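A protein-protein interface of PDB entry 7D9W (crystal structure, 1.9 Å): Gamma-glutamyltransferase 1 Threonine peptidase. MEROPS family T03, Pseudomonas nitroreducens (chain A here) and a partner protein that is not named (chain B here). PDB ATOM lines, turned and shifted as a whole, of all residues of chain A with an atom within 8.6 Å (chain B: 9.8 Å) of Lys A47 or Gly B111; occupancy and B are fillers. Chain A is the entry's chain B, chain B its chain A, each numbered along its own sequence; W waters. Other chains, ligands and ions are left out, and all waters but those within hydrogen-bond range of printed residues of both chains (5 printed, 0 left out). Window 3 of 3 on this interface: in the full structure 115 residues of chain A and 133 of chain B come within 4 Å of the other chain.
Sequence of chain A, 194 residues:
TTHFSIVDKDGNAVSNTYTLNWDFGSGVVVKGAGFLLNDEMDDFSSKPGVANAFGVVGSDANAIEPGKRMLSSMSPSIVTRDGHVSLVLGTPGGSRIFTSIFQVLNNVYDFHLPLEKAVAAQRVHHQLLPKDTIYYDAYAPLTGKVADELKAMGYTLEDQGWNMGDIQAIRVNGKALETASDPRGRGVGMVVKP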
ATOM      1  N   PHE A  44      -5.440   9.441  31.759  1.00  0.00           N
ATOM      2  CA  PHE A  44      -6.246   9.467  30.549  1.00  0.00           C
ATOM      3  C   PHE A  44      -5.353   9.240  29.331  1.00  0.00           C
ATOM      4  O   PHE A  44      -4.135   9.437  29.375  1.00  0.00           O
ATOM      5  CB  PHE A  44      -6.967  10.808  30.355  1.00  0.00           C
ATOM      6  CG  PHE A  44      -8.169  11.014  31.235  1.00  0.00           C
ATOM      7  CD1 PHE A  44      -9.273  10.183  31.129  1.00  0.00           C
ATOM      8  CD2 PHE A  44      -8.223  12.080  32.125  1.00  0.00           C
ATOM      9  CE1 PHE A  44     -10.386  10.378  31.911  1.00  0.00           C
ATOM     10  CE2 PHE A  44      -9.344  12.284  32.917  1.00  0.00           C
ATOM     11  CZ  PHE A  44     -10.428  11.434  32.806  1.00  0.00           C
ATOM     12  N   SER A  45      -5.969   8.857  28.220  1.00  0.00           N
ATOM     13  CA  SER A  45      -5.269   8.911  26.946  1.00  0.00           C
ATOM     14  C   SER A  45      -5.385  10.338  26.420  1.00  0.00           C
ATOM     15  O   SER A  45      -6.497  10.849  26.245  1.00  0.00           O
ATOM     16  CB  SER A  45      -5.843   7.913  25.952  1.00  0.00           C
ATOM     17  OG  SER A  45      -5.269   8.134  24.674  1.00  0.00           O
ATOM     18  N   SER A  46      -4.245  10.998  26.218  1.00  0.00           N
ATOM     19  CA  SER A  46      -4.253  12.372  25.730  1.00  0.00           C
ATOM     20  C   SER A  46      -4.445  12.449  24.222  1.00  0.00           C
ATOM     21  O   SER A  46      -4.809  13.512  23.707  1.00  0.00           O
ATOM     22  CB  SER A  46      -2.950  13.078  26.111  1.00  0.00           C
ATOM     23  OG  SER A  46      -2.838  13.234  27.512  1.00  0.00           O
ATOM     24  N   LYS A  47      -4.216  11.352  23.515  1.00  0.00           N
ATOM     25  CA  LYS A  47      -4.196  11.314  22.058  1.00  0.00           C
ATOM     26  C   LYS A  47      -4.105   9.840  21.683  1.00  0.00           C
ATOM     27  O   LYS A  47      -3.248   9.122  22.209  1.00  0.00           O
ATOM     28  CB  LYS A  47      -3.023  12.126  21.519  1.00  0.00           C
ATOM     29  CG  LYS A  47      -2.785  12.024  20.020  1.00  0.00           C
ATOM     30  CD  LYS A  47      -1.732  13.050  19.587  1.00  0.00           C
ATOM     31  CE  LYS A  47      -1.622  13.169  18.078  1.00  0.00           C
ATOM     32  N   PRO A  48      -4.974   9.342  20.809  1.00  0.00           N
ATOM     33  CA  PRO A  48      -4.998   7.897  20.553  1.00  0.00           C
ATOM     34  C   PRO A  48      -3.645   7.386  20.079  1.00  0.00           C
ATOM     35  O   PRO A  48      -3.024   7.958  19.181  1.00  0.00           O
ATOM     36  CB  PRO A  48      -6.080   7.747  19.475  1.00  0.00           C
ATOM     37  N   GLY A  49      -3.185   6.301  20.705  1.00  0.00           N
ATOM     38  CA  GLY A  49      -1.949   5.653  20.323  1.00  0.00           C
ATOM     39  C   GLY A  49      -0.691   6.211  20.953  1.00  0.00           C
ATOM     40  O   GLY A  49       0.386   5.632  20.758  1.00  0.00           O
ATOM     41  N   VAL A  50      -0.784   7.314  21.693  1.00  0.00           N
ATOM     42  CA  VAL A  50       0.368   7.938  22.332  1.00  0.00           C
ATOM     43  C   VAL A  50       0.446   7.445  23.770  1.00  0.00           C
ATOM     44  O   VAL A  50      -0.544   7.509  24.511  1.00  0.00           O
ATOM     45  CB  VAL A  50       0.278   9.471  22.282  1.00  0.00           C
ATOM     46  CG1 VAL A  50       1.323  10.099  23.204  1.00  0.00           C
ATOM     47  CG2 VAL A  50       0.445   9.967  20.859  1.00  0.00           C
ATOM     48  N   ALA A  51       1.617   6.956  24.163  1.00  0.00           N
ATOM     49  CA  ALA A  51       1.808   6.384  25.485  1.00  0.00           C
ATOM     50  C   ALA A  51       1.933   7.479  26.536  1.00  0.00           C
ATOM     51  O   ALA A  51       2.482   8.555  26.282  1.00  0.00           O
ATOM     52  CB  ALA A  51       3.059   5.504  25.501  1.00  0.00           C
ATOM     53  N   ASN A  52       1.412   7.190  27.733  1.00  0.00           N
ATOM     54  CA  ASN A  52       1.548   8.089  28.870  1.00  0.00           C
ATOM     55  C   ASN A  52       2.840   7.764  29.629  1.00  0.00           C
ATOM     56  O   ASN A  52       3.717   7.066  29.116  1.00  0.00           O
ATOM     57  CB  ASN A  52       0.312   7.997  29.775  1.00  0.00           C
ATOM     58  CG  ASN A  52       0.272   6.711  30.598  1.00  0.00           C
ATOM     59  OD1 ASN A  52       1.100   5.817  30.428  1.00  0.00           O
ATOM     60  ND2 ASN A  52      -0.700   6.622  31.499  1.00  0.00           N
ATOM     61  N   VAL A  56       1.542   3.060  28.602  1.00  0.00           N
ATOM     62  CA  VAL A  56       0.284   2.447  28.194  1.00  0.00           C
ATOM     63  C   VAL A  56      -0.489   3.427  27.326  1.00  0.00           C
ATOM     64  O   VAL A  56      -0.340   4.649  27.440  1.00  0.00           O
ATOM     65  CB  VAL A  56      -0.547   1.988  29.412  1.00  0.00           C
ATOM     66  CG1 VAL A  56       0.172   0.833  30.121  1.00  0.00           C
ATOM     67  CG2 VAL A  56      -0.791   3.132  30.368  1.00  0.00           C
ATOM     68  N   VAL A  57      -1.310   2.880  26.432  1.00  0.00           N
ATOM     69  CA  VAL A  57      -2.009   3.666  25.430  1.00  0.00           C
ATOM     70  C   VAL A  57      -3.512   3.474  25.607  1.00  0.00           C
ATOM     71  O   VAL A  57      -3.974   2.637  26.385  1.00  0.00           O
ATOM     72  CB  VAL A  57      -1.580   3.298  23.996  1.00  0.00           C
ATOM     73  CG1 VAL A  57      -0.096   3.578  23.793  1.00  0.00           C
ATOM     74  CG2 VAL A  57      -1.894   1.839  23.702  1.00  0.00           C
ATOM     75  N   GLY A  58      -4.277   4.274  24.867  1.00  0.00           N
ATOM     76  CA  GLY A  58      -5.724   4.163  24.928  1.00  0.00           C
ATOM     77  C   GLY A  58      -6.350   4.755  23.685  1.00  0.00           C
ATOM     78  O   GLY A  58      -5.670   5.179  22.747  1.00  0.00           O
ATOM     79  N   SER A  59      -7.680   4.773  23.694  1.00  0.00           N
ATOM     80  CA  SER A  59      -8.457   5.321  22.590  1.00  0.00           C
ATOM     81  C   SER A  59      -9.640   6.084  23.181  1.00  0.00           C
ATOM     82  O   SER A  59      -9.458   6.897  24.092  1.00  0.00           O
ATOM     83  CB  SER A  59      -8.895   4.206  21.647  1.00  0.00           C
ATOM     84  OG  SER A  59      -9.319   4.744  20.407  1.00  0.00           O
ATOM     85  N   ASP A  60     -10.853   5.824  22.696  1.00  0.00           N
ATOM     86  CA  ASP A  60     -11.994   6.619  23.144  1.00  0.00           C
ATOM     87  C   ASP A  60     -12.464   6.215  24.539  1.00  0.00           C
ATOM     88  O   ASP A  60     -12.884   7.074  25.323  1.00  0.00           O
ATOM     89  CB  ASP A  60     -13.141   6.502  22.137  1.00  0.00           C
ATOM     90  CG  ASP A  60     -13.018   7.501  20.994  1.00  0.00           C
ATOM     91  N   ASN A  62     -10.981   5.613  27.206  1.00  0.00           N
ATOM     92  CA  ASN A  62     -10.246   6.310  28.255  1.00  0.00           C
ATOM     93  C   ASN A  62      -9.831   7.711  27.822  1.00  0.00           C
ATOM     94  O   ASN A  62      -8.863   8.265  28.348  1.00  0.00           O
ATOM     95  CB  ASN A  62      -9.038   5.465  28.671  1.00  0.00           C
ATOM     96  CG  ASN A  62      -8.348   5.986  29.912  1.00  0.00           C
ATOM     97  OD1 ASN A  62      -9.001   6.374  30.887  1.00  0.00           O
ATOM     98  ND2 ASN A  62      -7.020   5.964  29.902  1.00  0.00           N
ATOM     99  N   ALA A  63     -10.543   8.292  26.862  1.00  0.00           N
ATOM    100  CA  ALA A  63     -10.294   9.677  26.501  1.00  0.00           C
ATOM    101  C   ALA A  63     -10.789  10.600  27.612  1.00  0.00           C
ATOM    102  O   ALA A  63     -11.623  10.227  28.447  1.00  0.00           O
ATOM    103  CB  ALA A  63     -10.974  10.017  25.176  1.00  0.00           C
ATOM    104  N   ILE A  64     -10.253  11.821  27.622  1.00  0.00           N
ATOM    105  CA  ILE A  64     -10.646  12.807  28.620  1.00  0.00           C
ATOM    106  C   ILE A  64     -12.084  13.249  28.374  1.00  0.00           C
ATOM    107  O   ILE A  64     -12.451  13.615  27.249  1.00  0.00           O
ATOM    108  CB  ILE A  64      -9.704  14.023  28.589  1.00  0.00           C
ATOM    109  CG1 ILE A  64      -8.270  13.618  28.918  1.00  0.00           C
ATOM    110  CG2 ILE A  64     -10.212  15.114  29.549  1.00  0.00           C
ATOM    111  CD1 ILE A  64      -7.230  14.601  28.409  1.00  0.00           C
ATOM    112  N   THR B 102     -11.243  18.932  28.576  1.00  0.00           N
ATOM    113  CA  THR B 102     -11.630  18.588  27.216  1.00  0.00           C
ATOM    114  C   THR B 102     -10.675  17.542  26.652  1.00  0.00           C
ATOM    115  O   THR B 102      -9.527  17.410  27.085  1.00  0.00           O
ATOM    116  CB  THR B 102     -11.637  19.804  26.268  1.00  0.00           C
ATOM    117  OG1 THR B 102     -10.363  20.465  26.323  1.00  0.00           O
ATOM    118  CG2 THR B 102     -12.742  20.784  26.626  1.00  0.00           C
ATOM    119  N   LYS B 103     -11.166  16.819  25.647  1.00  0.00           N
ATOM    120  CA  LYS B 103     -10.401  15.745  25.019  1.00  0.00           C
ATOM    121  C   LYS B 103      -9.007  16.190  24.593  1.00  0.00           C
ATOM    122  O   LYS B 103      -8.032  15.449  24.765  1.00  0.00           O
ATOM    123  CB  LYS B 103     -11.195  15.235  23.812  1.00  0.00           C
ATOM    124  CG  LYS B 103     -10.556  14.127  23.014  1.00  0.00           C
ATOM    125  CD  LYS B 103     -11.529  13.633  21.948  1.00  0.00           C
ATOM    126  N   THR B 104      -8.891  17.399  24.046  1.00  0.00           N
ATOM    127  CA  THR B 104      -7.656  17.861  23.429  1.00  0.00           C
ATOM    128  C   THR B 104      -6.884  18.848  24.303  1.00  0.00           C
ATOM    129  O   THR B 104      -6.014  19.565  23.791  1.00  0.00           O
ATOM    130  CB  THR B 104      -7.969  18.502  22.077  1.00  0.00           C
ATOM    131  OG1 THR B 104      -8.857  19.614  22.267  1.00  0.00           O
ATOM    132  CG2 THR B 104      -8.636  17.496  21.150  1.00  0.00           C
ATOM    133  N   MET B 105      -7.158  18.878  25.609  1.00  0.00           N
ATOM    134  CA  MET B 105      -6.636  19.951  26.446  1.00  0.00           C
ATOM    135  C   MET B 105      -5.115  19.943  26.568  1.00  0.00           C
ATOM    136  O   MET B 105      -4.537  20.971  26.938  1.00  0.00           O
ATOM    137  CB  MET B 105      -7.242  19.884  27.851  1.00  0.00           C
ATOM    138  CG  MET B 105      -7.122  18.531  28.539  1.00  0.00           C
ATOM    139  SD  MET B 105      -7.935  18.471  30.157  1.00  0.00           S
ATOM    140  CE  MET B 105      -7.034  19.721  31.074  1.00  0.00           C
ATOM    141  N   TYR B 106      -4.450  18.824  26.277  1.00  0.00           N
ATOM    142  CA  TYR B 106      -2.999  18.752  26.390  1.00  0.00           C
ATOM    143  C   TYR B 106      -2.289  18.738  25.040  1.00  0.00           C
ATOM    144  O   TYR B 106      -1.095  18.426  24.983  1.00  0.00           O
ATOM    145  CB  TYR B 106      -2.581  17.516  27.190  1.00  0.00           C
ATOM    146  CG  TYR B 106      -3.154  17.473  28.580  1.00  0.00           C
ATOM    147  CD1 TYR B 106      -2.898  18.495  29.488  1.00  0.00           C
ATOM    148  CD2 TYR B 106      -3.949  16.415  28.989  1.00  0.00           C
ATOM    149  CE1 TYR B 106      -3.419  18.459  30.763  1.00  0.00           C
ATOM    150  CE2 TYR B 106      -4.473  16.372  30.262  1.00  0.00           C
ATOM    151  CZ  TYR B 106      -4.205  17.394  31.143  1.00  0.00           C
ATOM    152  OH  TYR B 106      -4.732  17.345  32.413  1.00  0.00           O
ATOM    153  N   LEU B 107      -2.984  19.065  23.959  1.00  0.00           N
ATOM    154  CA  LEU B 107      -2.376  19.153  22.639  1.00  0.00           C
ATOM    155  C   LEU B 107      -2.043  20.607  22.320  1.00  0.00           C
ATOM    156  O   LEU B 107      -2.743  21.529  22.749  1.00  0.00           O
ATOM    157  CB  LEU B 107      -3.309  18.578  21.571  1.00  0.00           C
ATOM    158  CG  LEU B 107      -3.863  17.174  21.824  1.00  0.00           C
ATOM    159  CD1 LEU B 107      -4.650  16.673  20.616  1.00  0.00           C
ATOM    160  CD2 LEU B 107      -2.750  16.197  22.173  1.00  0.00           C
ATOM    161  N   ASN B 108      -0.960  20.808  21.570  1.00  0.00           N
ATOM    162  CA  ASN B 108      -0.559  22.153  21.185  1.00  0.00           C
ATOM    163  C   ASN B 108      -1.195  22.511  19.839  1.00  0.00           C
ATOM    164  O   ASN B 108      -2.047  21.790  19.316  1.00  0.00           O
ATOM    165  CB  ASN B 108       0.967  22.304  21.161  1.00  0.00           C
ATOM    166  CG  ASN B 108       1.656  21.331  20.215  1.00  0.00           C
ATOM    167  OD1 ASN B 108       1.089  20.901  19.210  1.00  0.00           O
ATOM    168  ND2 ASN B 108       2.911  21.017  20.518  1.00  0.00           N
ATOM    169  N   GLU B 109      -0.786  23.642  19.262  1.00  0.00           N
ATOM    170  CA  GLU B 109      -1.408  24.098  18.025  1.00  0.00           C
ATOM    171  C   GLU B 109      -1.038  23.234  16.826  1.00  0.00           C
ATOM    172  O   GLU B 109      -1.667  23.377  15.772  1.00  0.00           O
ATOM    173  CB  GLU B 109      -1.033  25.558  17.758  1.00  0.00           C
ATOM    174  CG  GLU B 109      -1.307  26.516  18.924  1.00  0.00           C
ATOM    175  CD  GLU B 109      -2.782  26.613  19.324  1.00  0.00           C
ATOM    176  OE1 GLU B 109      -3.606  25.801  18.854  1.00  0.00           O
ATOM    177  OE2 GLU B 109      -3.124  27.518  20.115  1.00  0.00           O
ATOM    178  N   LYS B 110      -0.046  22.351  16.954  1.00  0.00           N
ATOM    179  CA  LYS B 110       0.303  21.400  15.907  1.00  0.00           C
ATOM    180  C   LYS B 110      -0.313  20.027  16.148  1.00  0.00           C
ATOM    181  O   LYS B 110       0.029  19.070  15.445  1.00  0.00           O
ATOM    182  CB  LYS B 110       1.824  21.275  15.789  1.00  0.00           C
ATOM    183  N   GLY B 111      -1.214  19.907  17.120  1.00  0.00           N
ATOM    184  CA  GLY B 111      -1.828  18.634  17.426  1.00  0.00           C
ATOM    185  C   GLY B 111      -0.955  17.685  18.212  1.00  0.00           C
ATOM    186  O   GLY B 111      -1.286  16.495  18.296  1.00  0.00           O
ATOM    187  N   GLU B 112       0.135  18.178  18.790  1.00  0.00           N
ATOM    188  CA  GLU B 112       1.089  17.367  19.527  1.00  0.00           C
ATOM    189  C   GLU B 112       0.750  17.377  21.011  1.00  0.00           C
ATOM    190  O   GLU B 112       0.262  18.376  21.537  1.00  0.00           O
ATOM    191  CB  GLU B 112       2.501  17.928  19.362  1.00  0.00           C
ATOM    192  CG  GLU B 112       3.001  18.093  17.951  1.00  0.00           C
ATOM    193  CD  GLU B 112       4.367  18.763  17.922  1.00  0.00           C
ATOM    194  OE1 GLU B 112       4.648  19.592  18.823  1.00  0.00           O
ATOM    195  OE2 GLU B 112       5.166  18.448  17.026  1.00  0.00           O
ATOM    196  N   VAL B 113       1.058  16.276  21.699  1.00  0.00           N
ATOM    197  CA  VAL B 113       0.961  16.271  23.156  1.00  0.00           C
ATOM    198  C   VAL B 113       2.023  17.200  23.729  1.00  0.00           C
ATOM    199  O   VAL B 113       3.205  17.113  23.371  1.00  0.00           O
ATOM    200  CB  VAL B 113       1.112  14.847  23.709  1.00  0.00           C
ATOM    201  CG1 VAL B 113       1.073  14.864  25.232  1.00  0.00           C
ATOM    202  CG2 VAL B 113       0.016  13.952  23.163  1.00  0.00           C
ATOM    203  N   ILE B 114       1.610  18.097  24.620  1.00  0.00           N
ATOM    204  CA  ILE B 114       2.538  19.045  25.230  1.00  0.00           C
ATOM    205  C   ILE B 114       3.270  18.343  26.369  1.00  0.00           C
ATOM    206  O   ILE B 114       2.644  17.842  27.308  1.00  0.00           O
ATOM    207  CB  ILE B 114       1.804  20.294  25.735  1.00  0.00           C
ATOM    208  CG1 ILE B 114       1.280  21.120  24.561  1.00  0.00           C
ATOM    209  CG2 ILE B 114       2.736  21.155  26.571  1.00  0.00           C
ATOM    210  CD1 ILE B 114       0.173  22.081  24.934  1.00  0.00           C
ATOM    211  N   SER B 118       0.296  17.294  31.355  1.00  0.00           N
ATOM    212  CA  SER B 118      -0.563  16.403  32.126  1.00  0.00           C
ATOM    213  C   SER B 118       0.137  15.838  33.356  1.00  0.00           C
ATOM    214  O   SER B 118      -0.469  15.054  34.096  1.00  0.00           O
ATOM    215  CB  SER B 118      -1.055  15.258  31.239  1.00  0.00           C
ATOM    216  OG  SER B 118       0.035  14.488  30.763  1.00  0.00           O
ATOM    217  N   ALA B 315      -6.055  -1.506  26.324  1.00  0.00           N
ATOM    218  CA  ALA B 315      -5.943  -0.265  25.570  1.00  0.00           C
ATOM    219  C   ALA B 315      -7.196   0.018  24.756  1.00  0.00           C
ATOM    220  O   ALA B 315      -7.536   1.185  24.525  1.00  0.00           O
ATOM    221  CB  ALA B 315      -4.720  -0.324  24.653  1.00  0.00           C
HETATM  222  O   HOH W   1      -9.355   3.460  25.637  1.00  0.00           O
HETATM  223  O   HOH W   2      -8.468  12.578  25.441  1.00  0.00           O
HETATM  224  O   HOH W   3      -0.398  14.216  27.849  1.00  0.00           O
HETATM  225  O   HOH W   4      -3.607   0.370  27.929  1.00  0.00           O
HETATM  226  O   HOH W   5      -5.453  16.076  25.217  1.00  0.00           O
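Of chain B, only Lys B103 (3.9 Å), Tyr B106 (3.7 Å) and Leu B107 (3.7 Å) come within 4 Å of Ser A46. Lys A47 touches just these residues of chain B: Gly B111 (3.4 Å) and Val B113 (3.9 Å). No residue of chain B comes within 4 Å of Gly A49. No residue of chain B comes within 4 Å of Val A50. Of the printed residues of chain B, Ser A59 touches Ala B315. Of the printed residues of chain A, Thr B102 touches Ile A64. Printed residues of chain A within 4 Å of Met B105: Ile A64 (3.9 Å). No residue of chain A comes within 4 Å of Lys B110. Ser B118 touches none of the printed residues of chain A. Printed residues of chain A within 4 Å of Ala B315: Val A57, Gly A58 and Ser A59. The nearest residue of chain B that does not touch Lys A47 is Leu B107 (4.1 Å). The nearest residue of chain A that does not touch Gly B111 is Ser A46 (7.1 Å).
SD of Met B105 lies within hydrogen-bond range of N of Thr B102, 3.7 Å away. N of Ile B114 is in hydrogen-bond range of O of Tyr B106 (2.7 Å). The backbone NH of Gly B111 lies within hydrogen-bond range of the side-chain amide oxygen of Asn B108. OG of Ser A45 sits at hydrogen-bond distance from O of Lys A47 (3.3 Å). The backbone carbonyl oxygen (O) of Gly A58 sits at hydrogen-bond distance from the backbone NH (N) of Gly A49, 3.4 Å away.
Water W3 bridges the side-chain hydroxyl of Ser A46 (2.7 Å) and the side-chain hydroxyl of Ser B118 (3.0 Å). Water W5 lies within hydrogen-bond range of O of Lys B103 (2.7 Å), O of Ser A46 (3.0 Å), N of Tyr B106 (3.1 Å) and N of Met B105 (3.3 Å). Water W2 lies within hydrogen-bond range of O of Ser A45, N of Ile A64 and O of Lys B103. Water W4 bridges O of Val A57 (2.8 Å) and N of Ala B315 (3.5 Å). Water W1 lies within hydrogen-bond range of N of Ser A59 (2.9 Å), O of Ala B315 (3.1 Å) and N of Asn A62 (3.1 Å).
OG of Ser A46 touches CD2 of Tyr B106 (3.7 Å). Ser A46 touches Leu B107 (O to CD2, 3.7 Å). Lys A47 touches Gly B111. CB of Lys A47 touches CG2 of Val B113 (3.9 Å). Val A57 touches Ala B315 (O to CB, 3.5 Å). Ala B315 touches Gly A58 (O to CA, 3.5 Å). Thr B102 touches Ile A64. Lys B103 touches Ile A64 (CA to O, 3.7 Å). Met B105 touches Ile A64 (CG to CD1, 3.9 Å). Ile A64 touches Tyr B106.
Hydrophobic or aromatic side chains of chain A within 4 Å of the printed part of chain B: Val A57 and Ile A64. Along chain A the printed residues that touch a printed residue of chain B span positions 46 to 64. Of the 15 printed residues of chain B, 8 touch a printed residue of chain A. Along chain B the printed residues that touch a printed residue of chain A span positions 102 to 315.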
